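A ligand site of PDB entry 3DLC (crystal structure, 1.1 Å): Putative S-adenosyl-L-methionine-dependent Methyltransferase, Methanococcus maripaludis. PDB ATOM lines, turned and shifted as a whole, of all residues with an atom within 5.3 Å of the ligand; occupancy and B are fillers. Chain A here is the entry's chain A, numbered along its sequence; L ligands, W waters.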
ATOM      1  N   PHE A   9      14.454  30.327  21.387  1.00  0.00           N
ATOM      2  CA  PHE A   9      14.413  29.991  19.957  1.00  0.00           C
ATOM      3  C   PHE A   9      13.059  30.166  19.293  1.00  0.00           C
ATOM      4  O   PHE A   9      12.800  29.657  18.202  1.00  0.00           O
ATOM      5  CB  PHE A   9      15.007  28.585  19.663  1.00  0.00           C
ATOM      6  CG  PHE A   9      16.217  28.267  20.523  1.00  0.00           C
ATOM      7  CD1 PHE A   9      17.303  29.122  20.548  1.00  0.00           C
ATOM      8  CD2 PHE A   9      16.271  27.097  21.248  1.00  0.00           C
ATOM      9  CE1 PHE A   9      18.419  28.843  21.327  1.00  0.00           C
ATOM     10  CE2 PHE A   9      17.403  26.789  22.027  1.00  0.00           C
ATOM     11  CZ  PHE A   9      18.449  27.666  22.056  1.00  0.00           C
ATOM     12  N   MET A  17      18.506  36.964  17.954  1.00  0.00           N
ATOM     13  CA  MET A  17      19.691  36.323  17.433  1.00  0.00           C
ATOM     14  C   MET A  17      20.076  36.918  16.066  1.00  0.00           C
ATOM     15  O   MET A  17      21.259  37.163  15.792  1.00  0.00           O
ATOM     16  CB  MET A  17      19.479  34.830  17.328  1.00  0.00           C
ATOM     17  CG  MET A  17      20.737  34.021  16.933  1.00  0.00           C
ATOM     18  SD  MET A  17      22.156  34.007  18.252  1.00  0.00           S
ATOM     19  CE  MET A  17      23.501  35.007  17.277  1.00  0.00           C
ATOM     20  N   SER A  21      23.493  38.801  15.190  1.00  0.00           N
ATOM     21  CA  SER A  21      24.248  38.180  14.114  1.00  0.00           C
ATOM     22  C   SER A  21      24.661  39.207  13.019  1.00  0.00           C
ATOM     23  O   SER A  21      25.699  39.116  12.386  1.00  0.00           O
ATOM     24  CB  SER A  21      23.364  37.079  13.495  1.00  0.00           C
ATOM     25  OG  SER A  21      23.961  36.526  12.345  1.00  0.00           O
ATOM     26  N   TYR A  29      31.802  35.784  11.774  1.00  0.00           N
ATOM     27  CA  TYR A  29      31.437  34.678  10.887  1.00  0.00           C
ATOM     28  C   TYR A  29      32.485  34.484   9.753  1.00  0.00           C
ATOM     29  O   TYR A  29      32.887  33.349   9.524  1.00  0.00           O
ATOM     30  CB  TYR A  29      30.001  34.802  10.395  1.00  0.00           C
ATOM     31  CG  TYR A  29      29.029  34.824  11.545  1.00  0.00           C
ATOM     32  CD1 TYR A  29      28.670  33.671  12.194  1.00  0.00           C
ATOM     33  CD2 TYR A  29      28.454  36.015  11.973  1.00  0.00           C
ATOM     34  CE1 TYR A  29      27.793  33.686  13.269  1.00  0.00           C
ATOM     35  CE2 TYR A  29      27.583  36.037  13.045  1.00  0.00           C
ATOM     36  CZ  TYR A  29      27.236  34.891  13.674  1.00  0.00           C
ATOM     37  OH  TYR A  29      26.332  34.943  14.720  1.00  0.00           O
ATOM     38  N   ASP A  49      25.758  22.686   8.578  1.00  0.00           N
ATOM     39  CA  ASP A  49      25.831  23.666   9.664  1.00  0.00           C
ATOM     40  C   ASP A  49      24.691  23.335  10.624  1.00  0.00           C
ATOM     41  O   ASP A  49      23.521  23.562  10.332  1.00  0.00           O
ATOM     42  CB  ASP A  49      25.714  25.068   9.060  1.00  0.00           C
ATOM     43  CG  ASP A  49      25.774  26.183  10.087  1.00  0.00           C
ATOM     44  OD1 ASP A  49      26.101  25.904  11.249  1.00  0.00           O
ATOM     45  OD2 ASP A  49      25.477  27.337   9.687  1.00  0.00           O
ATOM     46  N   ILE A  50      25.042  22.773  11.774  1.00  0.00           N
ATOM     47  CA  ILE A  50      24.066  22.311  12.753  1.00  0.00           C
ATOM     48  C   ILE A  50      23.741  23.435  13.733  1.00  0.00           C
ATOM     49  O   ILE A  50      24.626  24.020  14.346  1.00  0.00           O
ATOM     50  CB  ILE A  50      24.551  21.055  13.481  1.00  0.00           C
ATOM     51  CG1 ILE A  50      24.808  19.926  12.461  1.00  0.00           C
ATOM     52  CG2 ILE A  50      23.526  20.634  14.566  1.00  0.00           C
ATOM     53  CD1 ILE A  50      25.348  18.642  13.092  1.00  0.00           C
ATOM     54  N   GLY A  51      22.451  23.697  13.904  1.00  0.00           N
ATOM     55  CA  GLY A  51      21.999  24.799  14.715  1.00  0.00           C
ATOM     56  C   GLY A  51      22.345  26.108  14.044  1.00  0.00           C
ATOM     57  O   GLY A  51      22.879  27.032  14.672  1.00  0.00           O
ATOM     58  N   SER A  52      22.019  26.192  12.755  1.00  0.00           N
ATOM     59  CA  SER A  52      22.413  27.271  11.889  1.00  0.00           C
ATOM     60  C   SER A  52      21.792  28.634  12.246  1.00  0.00           C
ATOM     61  O   SER A  52      22.330  29.679  11.871  1.00  0.00           O
ATOM     62  CB  SER A  52      22.089  26.885  10.439  1.00  0.00           C
ATOM     63  OG  SER A  52      20.798  26.290  10.329  1.00  0.00           O
ATOM     64  N   GLY A  53      20.652  28.613  12.931  1.00  0.00           N
ATOM     65  CA  GLY A  53      20.059  29.839  13.396  1.00  0.00           C
ATOM     66  C   GLY A  53      19.704  30.755  12.238  1.00  0.00           C
ATOM     67  O   GLY A  53      19.159  30.327  11.240  1.00  0.00           O
ATOM     68  N   PRO A  54      20.021  32.062  12.350  1.00  0.00           N
ATOM     69  CA  PRO A  54      19.745  32.983  11.248  1.00  0.00           C
ATOM     70  C   PRO A  54      20.613  32.767   9.993  1.00  0.00           C
ATOM     71  O   PRO A  54      20.386  33.429   8.993  1.00  0.00           O
ATOM     72  CB  PRO A  54      20.034  34.358  11.847  1.00  0.00           C
ATOM     73  CG  PRO A  54      19.936  34.186  13.327  1.00  0.00           C
ATOM     74  CD  PRO A  54      20.436  32.785  13.562  1.00  0.00           C
ATOM     75  N   ALA A  56      24.172  32.889   9.596  1.00  0.00           N
ATOM     76  CA  ALA A  56      25.349  33.693   9.297  1.00  0.00           C
ATOM     77  C   ALA A  56      26.601  32.867   9.072  1.00  0.00           C
ATOM     78  O   ALA A  56      27.435  33.285   8.291  1.00  0.00           O
ATOM     79  CB  ALA A  56      25.575  34.769  10.357  1.00  0.00           C
ATOM     80  N   LEU A  72      20.928  23.200   9.158  1.00  0.00           N
ATOM     81  CA  LEU A  72      19.971  22.431   9.936  1.00  0.00           C
ATOM     82  C   LEU A  72      19.631  23.152  11.234  1.00  0.00           C
ATOM     83  O   LEU A  72      20.511  23.493  12.021  1.00  0.00           O
ATOM     84  CB  LEU A  72      20.612  21.081  10.283  1.00  0.00           C
ATOM     85  CG  LEU A  72      19.781  20.138  11.152  1.00  0.00           C
ATOM     86  CD1 LEU A  72      18.619  19.541  10.361  1.00  0.00           C
ATOM     87  CD2 LEU A  72      20.621  18.991  11.723  1.00  0.00           C
ATOM     88  N   ASP A  73      18.356  23.370  11.477  1.00  0.00           N
ATOM     89  CA  ASP A  73      17.923  23.981  12.737  1.00  0.00           C
ATOM     90  C   ASP A  73      16.546  23.448  13.116  1.00  0.00           C
ATOM     91  O   ASP A  73      15.707  23.228  12.246  1.00  0.00           O
ATOM     92  CB  ASP A  73      17.907  25.498  12.621  1.00  0.00           C
ATOM     93  CG  ASP A  73      17.986  26.188  13.978  1.00  0.00           C
ATOM     94  OD1 ASP A  73      16.999  26.156  14.730  1.00  0.00           O
ATOM     95  OD2 ASP A  73      19.066  26.740  14.308  1.00  0.00           O
ATOM     96  N   PHE A  74      16.327  23.233  14.398  1.00  0.00           N
ATOM     97  CA  PHE A  74      15.073  22.695  14.888  1.00  0.00           C
ATOM     98  C   PHE A  74      14.005  23.730  15.132  1.00  0.00           C
ATOM     99  O   PHE A  74      12.871  23.349  15.441  1.00  0.00           O
ATOM    100  CB  PHE A  74      15.264  21.739  16.105  1.00  0.00           C
ATOM    101  CG  PHE A  74      15.458  22.385  17.458  1.00  0.00           C
ATOM    102  CD1 PHE A  74      15.832  23.718  17.630  1.00  0.00           C
ATOM    103  CD2 PHE A  74      15.315  21.592  18.576  1.00  0.00           C
ATOM    104  CE1 PHE A  74      16.009  24.217  18.918  1.00  0.00           C
ATOM    105  CE2 PHE A  74      15.498  22.085  19.835  1.00  0.00           C
ATOM    106  CZ  PHE A  74      15.848  23.404  20.023  1.00  0.00           C
ATOM    107  N   SER A  75      14.316  25.008  14.937  1.00  0.00           N
ATOM    108  CA  SER A  75      13.364  26.090  15.166  1.00  0.00           C
ATOM    109  C   SER A  75      12.822  26.624  13.866  1.00  0.00           C
ATOM    110  O   SER A  75      13.563  27.201  13.043  1.00  0.00           O
ATOM    111  CB  SER A  75      14.011  27.220  15.965  1.00  0.00           C
ATOM    112  OG  SER A  75      13.176  28.356  15.893  1.00  0.00           O
ATOM    113  N   MET A  78      13.651  30.295  13.475  1.00  0.00           N
ATOM    114  CA  MET A  78      15.009  30.548  12.991  1.00  0.00           C
ATOM    115  C   MET A  78      15.047  30.304  11.488  1.00  0.00           C
ATOM    116  O   MET A  78      15.645  31.058  10.741  1.00  0.00           O
ATOM    117  CB  MET A  78      16.017  29.608  13.638  1.00  0.00           C
ATOM    118  CG  MET A  78      16.335  29.896  15.078  1.00  0.00           C
ATOM    119  SD  MET A  78      17.250  31.638  15.185  1.00  0.00           S
ATOM    120  CE  MET A  78      17.619  31.450  16.993  1.00  0.00           C
ATOM    121  N   GLY A 100      15.004  20.392  11.246  1.00  0.00           N
ATOM    122  CA  GLY A 100      15.272  19.134  11.911  1.00  0.00           C
ATOM    123  C   GLY A 100      16.162  19.324  13.105  1.00  0.00           C
ATOM    124  O   GLY A 100      16.658  20.390  13.403  1.00  0.00           O
ATOM    125  N   ASP A 101      16.369  18.216  13.792  1.00  0.00           N
ATOM    126  CA  ASP A 101      17.030  18.132  15.090  1.00  0.00           C
ATOM    127  C   ASP A 101      18.293  17.289  15.013  1.00  0.00           C
ATOM    128  O   ASP A 101      18.331  16.242  14.330  1.00  0.00           O
ATOM    129  CB  ASP A 101      16.021  17.473  16.072  1.00  0.00           C
ATOM    130  CG  ASP A 101      16.342  17.662  17.518  1.00  0.00           C
ATOM    131  OD1 ASP A 101      17.476  17.368  17.951  1.00  0.00           O
ATOM    132  OD2 ASP A 101      15.435  18.123  18.258  1.00  0.00           O
ATOM    133  N   VAL A 102      19.340  17.741  15.694  1.00  0.00           N
ATOM    134  CA  VAL A 102      20.612  17.036  15.759  1.00  0.00           C
ATOM    135  C   VAL A 102      20.442  15.592  16.274  1.00  0.00           C
ATOM    136  O   VAL A 102      21.261  14.733  16.009  1.00  0.00           O
ATOM    137  CB  VAL A 102      21.631  17.818  16.614  1.00  0.00           C
ATOM    138  CG1 VAL A 102      21.265  17.836  18.097  1.00  0.00           C
ATOM    139  CG2 VAL A 102      23.044  17.258  16.377  1.00  0.00           C
ATOM    140  N   HIS A 103      19.358  15.342  17.022  1.00  0.00           N
ATOM    141  CA  HIS A 103      19.155  14.005  17.574  1.00  0.00           C
ATOM    142  C   HIS A 103      18.507  13.048  16.591  1.00  0.00           C
ATOM    143  O   HIS A 103      18.356  11.863  16.899  1.00  0.00           O
ATOM    144  CB  HIS A 103      18.300  14.043  18.839  1.00  0.00           C
ATOM    145  CG  HIS A 103      18.901  14.857  19.933  1.00  0.00           C
ATOM    146  ND1 HIS A 103      18.622  16.189  20.089  1.00  0.00           N
ATOM    147  CD2 HIS A 103      19.825  14.542  20.871  1.00  0.00           C
ATOM    148  CE1 HIS A 103      19.304  16.648  21.129  1.00  0.00           C
ATOM    149  NE2 HIS A 103      20.046  15.682  21.614  1.00  0.00           N
ATOM    150  N   ARG A 118      28.059  26.389  15.496  1.00  0.00           N
ATOM    151  CA  ARG A 118      28.439  27.429  16.443  1.00  0.00           C
ATOM    152  C   ARG A 118      27.306  27.721  17.384  1.00  0.00           C
ATOM    153  O   ARG A 118      26.183  27.993  16.955  1.00  0.00           O
ATOM    154  CB  ARG A 118      28.832  28.732  15.729  1.00  0.00           C
ATOM    155  CG  ARG A 118      29.270  29.799  16.687  1.00  0.00           C
ATOM    156  CD  ARG A 118      29.467  31.196  16.021  1.00  0.00           C
ATOM    157  NE  ARG A 118      29.801  32.136  17.054  1.00  0.00           N
ATOM    158  CZ  ARG A 118      28.918  32.644  17.923  1.00  0.00           C
ATOM    159  NH1 ARG A 118      27.633  32.440  17.728  1.00  0.00           N
ATOM    160  NH2 ARG A 118      29.318  33.371  18.929  1.00  0.00           N
ATOM    161  N   GLY A 119      27.601  27.744  18.662  1.00  0.00           N
ATOM    162  CA  GLY A 119      26.621  28.188  19.628  1.00  0.00           C
ATOM    163  C   GLY A 119      25.394  27.344  19.851  1.00  0.00           C
ATOM    164  O   GLY A 119      24.420  27.876  20.373  1.00  0.00           O
ATOM    165  N   SER A 120      25.381  26.110  19.350  1.00  0.00           N
ATOM    166  CA  SER A 120      24.281  25.173  19.523  1.00  0.00           C
ATOM    167  C   SER A 120      24.551  24.043  20.514  1.00  0.00           C
ATOM    168  O   SER A 120      23.660  23.690  21.299  1.00  0.00           O
ATOM    169  CB  SER A 120      23.934  24.651  18.130  1.00  0.00           C
ATOM    170  OG  SER A 120      22.669  24.026  18.086  1.00  0.00           O
ATOM    171  N   PHE A 123      23.429  23.843  24.203  1.00  0.00           N
ATOM    172  CA  PHE A 123      21.999  23.695  24.523  1.00  0.00           C
ATOM    173  C   PHE A 123      21.479  22.265  24.359  1.00  0.00           C
ATOM    174  O   PHE A 123      20.402  21.957  24.873  1.00  0.00           O
ATOM    175  CB  PHE A 123      21.149  24.615  23.616  1.00  0.00           C
ATOM    176  CG  PHE A 123      21.427  26.071  23.784  1.00  0.00           C
ATOM    177  CD1 PHE A 123      21.035  26.754  24.923  1.00  0.00           C
ATOM    178  CD2 PHE A 123      22.073  26.787  22.801  1.00  0.00           C
ATOM    179  CE1 PHE A 123      21.280  28.155  25.015  1.00  0.00           C
ATOM    180  CE2 PHE A 123      22.299  28.124  22.903  1.00  0.00           C
ATOM    181  CZ  PHE A 123      21.948  28.793  24.027  1.00  0.00           C
ATOM    182  N   TRP A 124      22.180  21.404  23.656  1.00  0.00           N
ATOM    183  CA  TRP A 124      21.611  20.099  23.326  1.00  0.00           C
ATOM    184  C   TRP A 124      21.342  19.223  24.511  1.00  0.00           C
ATOM    185  O   TRP A 124      22.174  19.089  25.373  1.00  0.00           O
ATOM    186  CB  TRP A 124      22.503  19.297  22.345  1.00  0.00           C
ATOM    187  CG  TRP A 124      22.761  19.991  21.066  1.00  0.00           C
ATOM    188  CD1 TRP A 124      22.045  21.022  20.505  1.00  0.00           C
ATOM    189  CD2 TRP A 124      23.834  19.707  20.152  1.00  0.00           C
ATOM    190  NE1 TRP A 124      22.617  21.405  19.309  1.00  0.00           N
ATOM    191  CE2 TRP A 124      23.736  20.644  19.101  1.00  0.00           C
ATOM    192  CE3 TRP A 124      24.874  18.789  20.134  1.00  0.00           C
ATOM    193  CZ2 TRP A 124      24.641  20.643  18.044  1.00  0.00           C
ATOM    194  CZ3 TRP A 124      25.779  18.822  19.090  1.00  0.00           C
ATOM    195  CH2 TRP A 124      25.657  19.752  18.067  1.00  0.00           C
HETATM  196  N1  LIG L   1      24.778  29.139  14.627  1.00  0.00           N
HETATM  197  C1  LIG L   1      24.125  30.466  14.729  1.00  0.00           C
HETATM  198  C2  LIG L   1      25.160  31.529  14.985  1.00  0.00           C
HETATM  199  O1  LIG L   1      26.259  31.194  15.415  1.00  0.00           O
HETATM  200  O2  LIG L   1      24.844  32.699  14.802  1.00  0.00           O
HETATM  201  C3  LIG L   1      23.040  30.450  15.783  1.00  0.00           C
HETATM  202  C4  LIG L   1      23.492  30.191  17.188  1.00  0.00           C
HETATM  203  S1  LIG L   1      22.077  30.202  18.292  1.00  0.00           S
HETATM  204  C5  LIG L   1      22.961  30.762  19.718  1.00  0.00           C
HETATM  205  C6  LIG L   1      21.755  28.390  18.643  1.00  0.00           C
HETATM  206  C7  LIG L   1      20.880  27.587  17.633  1.00  0.00           C
HETATM  207  O3  LIG L   1      20.851  26.127  17.781  1.00  0.00           O
HETATM  208  C8  LIG L   1      19.414  28.092  17.544  1.00  0.00           C
HETATM  209  O4  LIG L   1      19.188  28.521  16.237  1.00  0.00           O
HETATM  210  C9  LIG L   1      18.596  26.848  17.893  1.00  0.00           C
HETATM  211  O5  LIG L   1      17.296  26.765  17.365  1.00  0.00           O
HETATM  212  C10 LIG L   1      19.531  25.708  17.446  1.00  0.00           C
HETATM  213  N2  LIG L   1      19.300  24.431  18.150  1.00  0.00           N
HETATM  214  C11 LIG L   1      19.293  24.231  19.510  1.00  0.00           C
HETATM  215  N3  LIG L   1      19.134  22.927  19.796  1.00  0.00           N
HETATM  216  C12 LIG L   1      19.014  22.269  18.597  1.00  0.00           C
HETATM  217  C13 LIG L   1      18.797  20.929  18.262  1.00  0.00           C
HETATM  218  N4  LIG L   1      18.583  19.945  19.145  1.00  0.00           N
HETATM  219  N5  LIG L   1      18.787  20.626  16.944  1.00  0.00           N
HETATM  220  C14 LIG L   1      18.940  21.591  15.981  1.00  0.00           C
HETATM  221  N6  LIG L   1      19.090  22.919  16.263  1.00  0.00           N
HETATM  222  C15 LIG L   1      19.141  23.208  17.567  1.00  0.00           C
HETATM  223  O   HOH W   1      18.144  19.474  22.330  1.00  0.00           O
HETATM  224  O   HOH W   2      18.412  22.318  22.445  1.00  0.00           O
HETATM  225  O   HOH W   3      25.832  26.754  13.713  1.00  0.00           O
HETATM  226  O   HOH W   4      23.458  33.640  12.466  1.00  0.00           O
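The side-chain hydroxyl (OH) of Tyr 29 is in hydrogen-bond range of an oxygen (O2) of the ligand (2.7 Å).
N of Val 102 is in hydrogen-bond range of N5 of the ligand, 3.2 Å away.
O of Arg 118 sits at hydrogen-bond distance from N1 of the ligand.
OG of Ser 120 is in hydrogen-bond range of O3 of the ligand.
The guanidinium group (NH1) of Arg 118 is in salt-bridge range of an oxygen (O1) of the ligand (3.0 Å).
A nitrogen (N1) of the ligand lies within hydrogen-bond range of the backbone carbonyl oxygen (O) of Gly 51 (2.8 Å).
The backbone NH (N) of Phe 74 lies within hydrogen-bond range of a nitrogen (N6) of the ligand (3.3 Å).
N4 of the ligand lies within hydrogen-bond range of OD1 of Asp 101, at 3.0 Å.
The side-chain carboxylate of Asp 73 lies within hydrogen-bond range of an oxygen (O4) of the ligand (2.6 Å).
Water W2 bridges N3 of the ligand (2.8 Å) and O of Phe 123 (3.2 Å).
Water W4 lies within hydrogen-bond range of O2 of the ligand, OG of Ser 21 and N of Ala 56.
Phe 9 touches the ligand.
Met 17 touches the ligand.
Ser 52 touches the ligand.
Gly 53 touches the ligand (CA to O4, 3.3 Å).
Ser 75 touches the ligand (CB to O5, 3.6 Å).
CG of Met 78 touches O4 of the ligand, 3.4 Å away.
Gly 100 touches the ligand (O to C14, 3.6 Å).
ND1 of His 103 touches N4 of the ligand, at 3.9 Å.
Gly 119 touches the ligand.
Trp 124 touches the ligand (CD1 to N3, 3.6 Å).
Hydrophobic or aromatic side chains within 4 Å of the ligand: Phe 9, Met 17, Tyr 29, Phe 74, Met 78, Val 102, His 103 and Trp 124.
18 residues have an atom within 4 Å of the ligand: Phe 9, Met 17, Tyr 29, Gly 51, Ser 52, Gly 53, Asp 73, Phe 74, Ser 75, Met 78, Gly 100, Asp 101, Val 102, His 103, Arg 118, Gly 119, Ser 120 and Trp 124.
The nearest printed residue that does not touch the ligand is Pro 54 (4.1 Å).
OG of Ser 75 is in hydrogen-bond range of N of Met 78 (3.1 Å).
The side-chain carboxylate (OD1) of Asp 101 sits at hydrogen-bond distance from a ring nitrogen (ND1) of His 103, 2.7 Å away.
The backbone NH of Phe 74 lies within hydrogen-bond range of the backbone carbonyl oxygen of Gly 100 (3.0 Å).
The backbone NH (N) of Ser 75 sits at hydrogen-bond distance from the side-chain carboxylate (OD1) of Asp 73, 2.9 Å away.
The backbone NH of Gly 51 sits at hydrogen-bond distance from the backbone carbonyl oxygen of Leu 72.
The backbone carbonyl oxygen (O) of Asp 73 lies within hydrogen-bond range of the backbone NH (N) of Gly 100 (3.1 Å).
OG of Ser 75 sits at hydrogen-bond distance from O of Phe 9.
The side-chain carboxylate (OD2) of Asp 73 lies within hydrogen-bond range of the backbone NH (N) of Gly 53.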
